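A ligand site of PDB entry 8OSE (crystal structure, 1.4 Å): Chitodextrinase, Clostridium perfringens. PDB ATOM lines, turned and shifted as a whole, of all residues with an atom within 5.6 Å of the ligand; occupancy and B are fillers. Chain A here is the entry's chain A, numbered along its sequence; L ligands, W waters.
O4 of the ligand sits at hydrogen-bond distance from OG1 of Thr 114 (3.0 Å). The side-chain hydroxyl (OH) of Tyr 236 lies within hydrogen-bond range of a nitrogen (N4) of the ligand (2.8 Å). N of Trp 113 lies within hydrogen-bond range of O2 of the ligand, 3.0 Å away.
The backbone NH (N) of Ala 208 lies close to the side-chain carboxylate (OD1) of Asp 151 (3.4 Å). The backbone carbonyl oxygen (O) of Asp 151 lies within hydrogen-bond range of the backbone NH (N) of Gly 112 (2.8 Å). The side-chain carboxylate of Asp 237 is in hydrogen-bond range of the side-chain hydroxyl of Tyr 294, 2.7 Å away. The side-chain carboxylate of Glu 153 lies close to the backbone NH of Trp 113 (3.4 Å). The side-chain hydroxyl (OH) of Tyr 13 lies within hydrogen-bond range of the side-chain carboxylate (OD2) of Asp 151 (2.8 Å).
OH of Tyr 13 touches C5 of the ligand, 3.4 Å away. Trp 17 touches the ligand. Gln 24 touches the ligand. Phe 44 touches the ligand (CZ to O2, 3.6 Å). CA of Gly 112 touches O2 of the ligand, at 3.3 Å. Asp 151 touches the ligand. OE2 of Glu 153 touches C7 of the ligand (3.4 Å). Met 234 touches the ligand. Tyr 294 touches the ligand. Trp 402 touches the ligand. The nearest printed residue that does not touch the ligand is Asp 237 (4.1 Å).
Water W3 lies within hydrogen-bond range of the side-chain carboxylate of Asp 237, an oxygen (O1) of the ligand and the guanidinium group of Arg 296.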
ATOM      1  N   TYR A  13      17.521  23.732 -14.552  1.00  0.00           N
ATOM      2  CA  TYR A  13      18.851  24.026 -15.059  1.00  0.00           C
ATOM      3  C   TYR A  13      18.807  24.602 -16.466  1.00  0.00           C
ATOM      4  O   TYR A  13      18.145  24.051 -17.362  1.00  0.00           O
ATOM      5  CB  TYR A  13      19.682  22.762 -15.103  1.00  0.00           C
ATOM      6  CG  TYR A  13      20.370  22.373 -13.813  1.00  0.00           C
ATOM      7  CD1 TYR A  13      21.525  23.026 -13.361  1.00  0.00           C
ATOM      8  CD2 TYR A  13      19.949  21.281 -13.078  1.00  0.00           C
ATOM      9  CE1 TYR A  13      22.162  22.640 -12.220  1.00  0.00           C
ATOM     10  CE2 TYR A  13      20.634  20.867 -11.924  1.00  0.00           C
ATOM     11  CZ  TYR A  13      21.725  21.544 -11.525  1.00  0.00           C
ATOM     12  OH  TYR A  13      22.381  21.113 -10.395  1.00  0.00           O
ATOM     13  N   TRP A  17      25.571  26.146 -22.974  1.00  0.00           N
ATOM     14  CA  TRP A  17      26.130  25.659 -24.228  1.00  0.00           C
ATOM     15  C   TRP A  17      25.081  25.329 -25.280  1.00  0.00           C
ATOM     16  O   TRP A  17      25.442  25.016 -26.422  1.00  0.00           O
ATOM     17  CB  TRP A  17      26.943  24.369 -23.954  1.00  0.00           C
ATOM     18  CG  TRP A  17      26.177  23.341 -23.120  1.00  0.00           C
ATOM     19  CD1 TRP A  17      25.359  22.332 -23.569  1.00  0.00           C
ATOM     20  CD2 TRP A  17      26.156  23.267 -21.696  1.00  0.00           C
ATOM     21  NE1 TRP A  17      24.817  21.647 -22.500  1.00  0.00           N
ATOM     22  CE2 TRP A  17      25.310  22.195 -21.344  1.00  0.00           C
ATOM     23  CE3 TRP A  17      26.789  24.000 -20.696  1.00  0.00           C
ATOM     24  CZ2 TRP A  17      25.065  21.845 -20.010  1.00  0.00           C
ATOM     25  CZ3 TRP A  17      26.563  23.639 -19.373  1.00  0.00           C
ATOM     26  CH2 TRP A  17      25.695  22.573 -19.046  1.00  0.00           C
ATOM     27  N   GLN A  24      21.272  20.155 -29.095  1.00  0.00           N
ATOM     28  CA  GLN A  24      20.607  20.807 -27.983  1.00  0.00           C
ATOM     29  C   GLN A  24      19.438  21.673 -28.443  1.00  0.00           C
ATOM     30  O   GLN A  24      18.791  22.327 -27.607  1.00  0.00           O
ATOM     31  CB  GLN A  24      21.639  21.642 -27.232  1.00  0.00           C
ATOM     32  CG  GLN A  24      22.878  20.925 -26.737  1.00  0.00           C
ATOM     33  CD  GLN A  24      22.657  20.031 -25.558  1.00  0.00           C
ATOM     34  OE1 GLN A  24      21.593  20.003 -24.990  1.00  0.00           O
ATOM     35  NE2 GLN A  24      23.659  19.265 -25.217  1.00  0.00           N
ATOM     36  N   PHE A  44      27.252  26.859 -16.371  1.00  0.00           N
ATOM     37  CA  PHE A  44      27.842  26.762 -15.056  1.00  0.00           C
ATOM     38  C   PHE A  44      28.868  27.868 -14.906  1.00  0.00           C
ATOM     39  O   PHE A  44      29.468  28.343 -15.869  1.00  0.00           O
ATOM     40  CB  PHE A  44      28.666  25.464 -14.913  1.00  0.00           C
ATOM     41  CG  PHE A  44      27.844  24.218 -14.736  1.00  0.00           C
ATOM     42  CD1 PHE A  44      27.178  23.985 -13.546  1.00  0.00           C
ATOM     43  CD2 PHE A  44      27.785  23.251 -15.720  1.00  0.00           C
ATOM     44  CE1 PHE A  44      26.421  22.837 -13.378  1.00  0.00           C
ATOM     45  CE2 PHE A  44      27.056  22.116 -15.550  1.00  0.00           C
ATOM     46  CZ  PHE A  44      26.366  21.912 -14.377  1.00  0.00           C
ATOM     47  N   GLY A 111      30.258  24.513 -10.421  1.00  0.00           N
ATOM     48  CA  GLY A 111      30.747  23.152 -10.393  1.00  0.00           C
ATOM     49  C   GLY A 111      30.218  22.314 -11.536  1.00  0.00           C
ATOM     50  O   GLY A 111      30.418  22.624 -12.705  1.00  0.00           O
ATOM     51  N   GLY A 112      29.546  21.208 -11.187  1.00  0.00           N
ATOM     52  CA  GLY A 112      29.149  20.210 -12.156  1.00  0.00           C
ATOM     53  C   GLY A 112      30.238  19.172 -12.369  1.00  0.00           C
ATOM     54  O   GLY A 112      31.353  19.263 -11.853  1.00  0.00           O
ATOM     55  N   TRP A 113      29.898  18.181 -13.183  1.00  0.00           N
ATOM     56  CA  TRP A 113      30.811  17.061 -13.389  1.00  0.00           C
ATOM     57  C   TRP A 113      32.159  17.511 -13.924  1.00  0.00           C
ATOM     58  O   TRP A 113      33.194  16.942 -13.569  1.00  0.00           O
ATOM     59  CB  TRP A 113      30.177  16.079 -14.366  1.00  0.00           C
ATOM     60  CG  TRP A 113      30.961  14.844 -14.652  1.00  0.00           C
ATOM     61  CD1 TRP A 113      31.471  14.487 -15.851  1.00  0.00           C
ATOM     62  CD2 TRP A 113      31.269  13.764 -13.751  1.00  0.00           C
ATOM     63  NE1 TRP A 113      32.120  13.293 -15.768  1.00  0.00           N
ATOM     64  CE2 TRP A 113      31.981  12.801 -14.499  1.00  0.00           C
ATOM     65  CE3 TRP A 113      30.981  13.506 -12.421  1.00  0.00           C
ATOM     66  CZ2 TRP A 113      32.415  11.611 -13.946  1.00  0.00           C
ATOM     67  CZ3 TRP A 113      31.418  12.327 -11.876  1.00  0.00           C
ATOM     68  CH2 TRP A 113      32.145  11.411 -12.625  1.00  0.00           C
ATOM     69  N   THR A 114      32.170  18.478 -14.834  1.00  0.00           N
ATOM     70  CA  THR A 114      33.432  18.929 -15.427  1.00  0.00           C
ATOM     71  C   THR A 114      33.908  20.257 -14.880  1.00  0.00           C
ATOM     72  O   THR A 114      34.859  20.804 -15.421  1.00  0.00           O
ATOM     73  CB  THR A 114      33.348  19.006 -16.954  1.00  0.00           C
ATOM     74  OG1 THR A 114      32.436  20.038 -17.311  1.00  0.00           O
ATOM     75  CG2 THR A 114      32.904  17.696 -17.528  1.00  0.00           C
ATOM     76  N   GLY A 115      33.232  20.815 -13.883  1.00  0.00           N
ATOM     77  CA  GLY A 115      33.606  22.071 -13.284  1.00  0.00           C
ATOM     78  C   GLY A 115      33.961  22.021 -11.818  1.00  0.00           C
ATOM     79  O   GLY A 115      34.028  23.049 -11.142  1.00  0.00           O
ATOM     80  N   ASP A 151      27.470  22.829  -6.761  1.00  0.00           N
ATOM     81  CA  ASP A 151      27.353  21.523  -7.386  1.00  0.00           C
ATOM     82  C   ASP A 151      28.702  20.816  -7.421  1.00  0.00           C
ATOM     83  O   ASP A 151      29.252  20.519  -8.481  1.00  0.00           O
ATOM     84  CB  ASP A 151      26.762  21.651  -8.801  1.00  0.00           C
ATOM     85  CG  ASP A 151      25.356  22.156  -8.797  1.00  0.00           C
ATOM     86  OD1 ASP A 151      24.731  22.382  -7.739  1.00  0.00           O
ATOM     87  OD2 ASP A 151      24.824  22.380  -9.939  1.00  0.00           O
ATOM     88  N   GLU A 153      31.043  17.858  -7.267  1.00  0.00           N
ATOM     89  CA  GLU A 153      30.917  16.432  -7.555  1.00  0.00           C
ATOM     90  C   GLU A 153      32.263  15.732  -7.417  1.00  0.00           C
ATOM     91  O   GLU A 153      32.982  15.597  -8.403  1.00  0.00           O
ATOM     92  CB  GLU A 153      30.330  16.243  -8.986  1.00  0.00           C
ATOM     93  CG  GLU A 153      28.938  16.878  -9.082  1.00  0.00           C
ATOM     94  CD  GLU A 153      28.144  16.421 -10.297  1.00  0.00           C
ATOM     95  OE1 GLU A 153      28.685  15.745 -11.194  1.00  0.00           O
ATOM     96  OE2 GLU A 153      26.944  16.820 -10.347  1.00  0.00           O
ATOM     97  N   ALA A 208      23.043  20.995  -5.157  1.00  0.00           N
ATOM     98  CA  ALA A 208      22.576  19.774  -5.789  1.00  0.00           C
ATOM     99  C   ALA A 208      23.541  18.665  -5.371  1.00  0.00           C
ATOM    100  O   ALA A 208      24.750  18.772  -5.611  1.00  0.00           O
ATOM    101  CB  ALA A 208      22.491  19.919  -7.315  1.00  0.00           C
ATOM    102  N   MET A 234      20.003  14.679  -6.546  1.00  0.00           N
ATOM    103  CA  MET A 234      20.184  14.285  -7.939  1.00  0.00           C
ATOM    104  C   MET A 234      19.744  12.837  -8.108  1.00  0.00           C
ATOM    105  O   MET A 234      20.530  11.911  -8.293  1.00  0.00           O
ATOM    106  CB  MET A 234      21.628  14.503  -8.390  1.00  0.00           C
ATOM    107  CG  MET A 234      21.999  15.967  -8.424  1.00  0.00           C
ATOM    108  SD  MET A 234      23.615  16.315  -9.161  1.00  0.00           S
ATOM    109  CE  MET A 234      24.603  15.577  -7.911  1.00  0.00           C
ATOM    110  N   TYR A 236      18.767  10.764 -10.224  1.00  0.00           N
ATOM    111  CA  TYR A 236      18.878  10.329 -11.613  1.00  0.00           C
ATOM    112  C   TYR A 236      20.322   9.882 -11.823  1.00  0.00           C
ATOM    113  O   TYR A 236      21.105   9.867 -10.891  1.00  0.00           O
ATOM    114  CB  TYR A 236      18.406  11.416 -12.578  1.00  0.00           C
ATOM    115  CG  TYR A 236      18.861  12.802 -12.284  1.00  0.00           C
ATOM    116  CD1 TYR A 236      20.207  13.119 -12.341  1.00  0.00           C
ATOM    117  CD2 TYR A 236      17.974  13.822 -11.985  1.00  0.00           C
ATOM    118  CE1 TYR A 236      20.650  14.421 -12.120  1.00  0.00           C
ATOM    119  CE2 TYR A 236      18.385  15.113 -11.779  1.00  0.00           C
ATOM    120  CZ  TYR A 236      19.729  15.417 -11.829  1.00  0.00           C
ATOM    121  OH  TYR A 236      20.146  16.714 -11.639  1.00  0.00           O
ATOM    122  N   ASP A 237      20.637   9.415 -13.026  1.00  0.00           N
ATOM    123  CA  ASP A 237      21.917   8.747 -13.241  1.00  0.00           C
ATOM    124  C   ASP A 237      22.097   7.534 -12.343  1.00  0.00           C
ATOM    125  O   ASP A 237      23.210   7.122 -12.033  1.00  0.00           O
ATOM    126  CB  ASP A 237      23.115   9.688 -13.155  1.00  0.00           C
ATOM    127  CG  ASP A 237      23.243  10.605 -14.346  1.00  0.00           C
ATOM    128  OD1 ASP A 237      22.721  10.332 -15.439  1.00  0.00           O
ATOM    129  OD2 ASP A 237      23.954  11.616 -14.179  1.00  0.00           O
ATOM    130  N   TYR A 294      16.169  13.940 -19.794  1.00  0.00           N
ATOM    131  CA  TYR A 294      17.096  13.266 -20.694  1.00  0.00           C
ATOM    132  C   TYR A 294      16.977  11.784 -20.403  1.00  0.00           C
ATOM    133  O   TYR A 294      16.381  11.383 -19.389  1.00  0.00           O
ATOM    134  CB  TYR A 294      18.547  13.744 -20.522  1.00  0.00           C
ATOM    135  CG  TYR A 294      19.152  13.319 -19.211  1.00  0.00           C
ATOM    136  CD1 TYR A 294      18.845  13.989 -18.047  1.00  0.00           C
ATOM    137  CD2 TYR A 294      20.005  12.224 -19.125  1.00  0.00           C
ATOM    138  CE1 TYR A 294      19.388  13.625 -16.852  1.00  0.00           C
ATOM    139  CE2 TYR A 294      20.558  11.831 -17.919  1.00  0.00           C
ATOM    140  CZ  TYR A 294      20.251  12.531 -16.775  1.00  0.00           C
ATOM    141  OH  TYR A 294      20.726  12.182 -15.540  1.00  0.00           O
ATOM    142  N   ARG A 296      18.994   7.670 -20.697  1.00  0.00           N
ATOM    143  CA  ARG A 296      20.163   6.806 -20.941  1.00  0.00           C
ATOM    144  C   ARG A 296      19.646   5.459 -21.439  1.00  0.00           C
ATOM    145  O   ARG A 296      18.493   5.110 -21.186  1.00  0.00           O
ATOM    146  CB  ARG A 296      21.062   6.639 -19.733  1.00  0.00           C
ATOM    147  CG  ARG A 296      21.719   7.942 -19.269  1.00  0.00           C
ATOM    148  CD  ARG A 296      22.691   7.749 -18.117  1.00  0.00           C
ATOM    149  NE  ARG A 296      23.415   8.975 -17.818  1.00  0.00           N
ATOM    150  CZ  ARG A 296      24.385   9.504 -18.557  1.00  0.00           C
ATOM    151  NH1 ARG A 296      24.867   8.878 -19.600  1.00  0.00           N
ATOM    152  NH2 ARG A 296      24.860  10.700 -18.236  1.00  0.00           N
ATOM    153  N   ASP A 325      28.505  12.244 -25.665  1.00  0.00           N
ATOM    154  CA  ASP A 325      29.631  13.150 -25.567  1.00  0.00           C
ATOM    155  C   ASP A 325      30.599  12.962 -26.720  1.00  0.00           C
ATOM    156  O   ASP A 325      30.832  11.845 -27.186  1.00  0.00           O
ATOM    157  CB  ASP A 325      30.366  12.944 -24.237  1.00  0.00           C
ATOM    158  CG  ASP A 325      29.575  13.444 -23.050  1.00  0.00           C
ATOM    159  OD1 ASP A 325      29.009  14.557 -23.135  1.00  0.00           O
ATOM    160  OD2 ASP A 325      29.519  12.716 -22.032  1.00  0.00           O
ATOM    161  N   TRP A 402      16.992  18.569 -14.472  1.00  0.00           N
ATOM    162  CA  TRP A 402      18.113  18.574 -15.425  1.00  0.00           C
ATOM    163  C   TRP A 402      17.526  17.958 -16.695  1.00  0.00           C
ATOM    164  O   TRP A 402      17.223  16.766 -16.702  1.00  0.00           O
ATOM    165  CB  TRP A 402      19.335  17.766 -14.988  1.00  0.00           C
ATOM    166  CG  TRP A 402      20.399  17.808 -16.051  1.00  0.00           C
ATOM    167  CD1 TRP A 402      20.426  17.083 -17.189  1.00  0.00           C
ATOM    168  CD2 TRP A 402      21.546  18.689 -16.095  1.00  0.00           C
ATOM    169  NE1 TRP A 402      21.533  17.422 -17.936  1.00  0.00           N
ATOM    170  CE2 TRP A 402      22.213  18.420 -17.312  1.00  0.00           C
ATOM    171  CE3 TRP A 402      22.049  19.668 -15.252  1.00  0.00           C
ATOM    172  CZ2 TRP A 402      23.364  19.090 -17.677  1.00  0.00           C
ATOM    173  CZ3 TRP A 402      23.211  20.321 -15.628  1.00  0.00           C
ATOM    174  CH2 TRP A 402      23.846  20.029 -16.840  1.00  0.00           C
HETATM  175  N1  LIG L   1      25.783  17.035 -15.286  1.00  0.00           N
HETATM  176  C1  LIG L   1      24.686  16.263 -15.608  1.00  0.00           C
HETATM  177  O1  LIG L   1      24.678  15.563 -16.610  1.00  0.00           O
HETATM  178  N2  LIG L   1      23.606  16.319 -14.748  1.00  0.00           N
HETATM  179  C2  LIG L   1      23.654  17.138 -13.650  1.00  0.00           C
HETATM  180  C3  LIG L   1      24.747  17.876 -13.357  1.00  0.00           C
HETATM  181  C4  LIG L   1      25.914  17.848 -14.167  1.00  0.00           C
HETATM  182  O2  LIG L   1      26.989  18.409 -13.934  1.00  0.00           O
HETATM  183  N3  LIG L   1      24.426  18.577 -12.218  1.00  0.00           N
HETATM  184  C5  LIG L   1      23.172  18.225 -11.898  1.00  0.00           C
HETATM  185  N4  LIG L   1      22.661  17.326 -12.736  1.00  0.00           N
HETATM  186  N5  LIG L   1      28.299  19.022 -19.106  1.00  0.00           N
HETATM  187  C6  LIG L   1      28.149  17.914 -18.146  1.00  0.00           C
HETATM  188  C7  LIG L   1      25.265  19.503 -11.473  1.00  0.00           C
HETATM  189  C8  LIG L   1      27.248  19.225 -23.562  1.00  0.00           C
HETATM  190  C9  LIG L   1      22.484  15.400 -14.961  1.00  0.00           C
HETATM  191  C10 LIG L   1      29.969  22.307 -19.092  1.00  0.00           C
HETATM  192  O3  LIG L   1      27.070  17.890 -20.664  1.00  0.00           O
HETATM  193  O4  LIG L   1      29.399  20.156 -17.482  1.00  0.00           O
HETATM  194  C11 LIG L   1      28.646  21.221 -22.938  1.00  0.00           C
HETATM  195  C12 LIG L   1      26.936  16.940 -16.183  1.00  0.00           C
HETATM  196  C13 LIG L   1      27.005  18.100 -17.170  1.00  0.00           C
HETATM  197  N6  LIG L   1      29.218  21.790 -21.896  1.00  0.00           N
HETATM  198  C14 LIG L   1      27.779  18.858 -20.390  1.00  0.00           C
HETATM  199  C15 LIG L   1      29.024  20.094 -18.645  1.00  0.00           C
HETATM  200  C16 LIG L   1      28.892  20.974 -20.861  1.00  0.00           C
HETATM  201  C17 LIG L   1      28.150  19.918 -21.275  1.00  0.00           C
HETATM  202  N7  LIG L   1      27.983  20.093 -22.635  1.00  0.00           N
HETATM  203  N8  LIG L   1      29.299  21.108 -19.558  1.00  0.00           N
HETATM  204  O   HOH W   1      26.106  16.035 -24.385  1.00  0.00           O
HETATM  205  O   HOH W   2      32.457  20.104 -20.122  1.00  0.00           O
HETATM  206  O   HOH W   3      24.955  12.785 -16.344  1.00  0.00           O
HETATM  207  O   HOH W   4      22.963  14.252 -19.315  1.00  0.00           O
HETATM  208  O   HOH W   5      30.937  18.121 -21.220  1.00  0.00           O
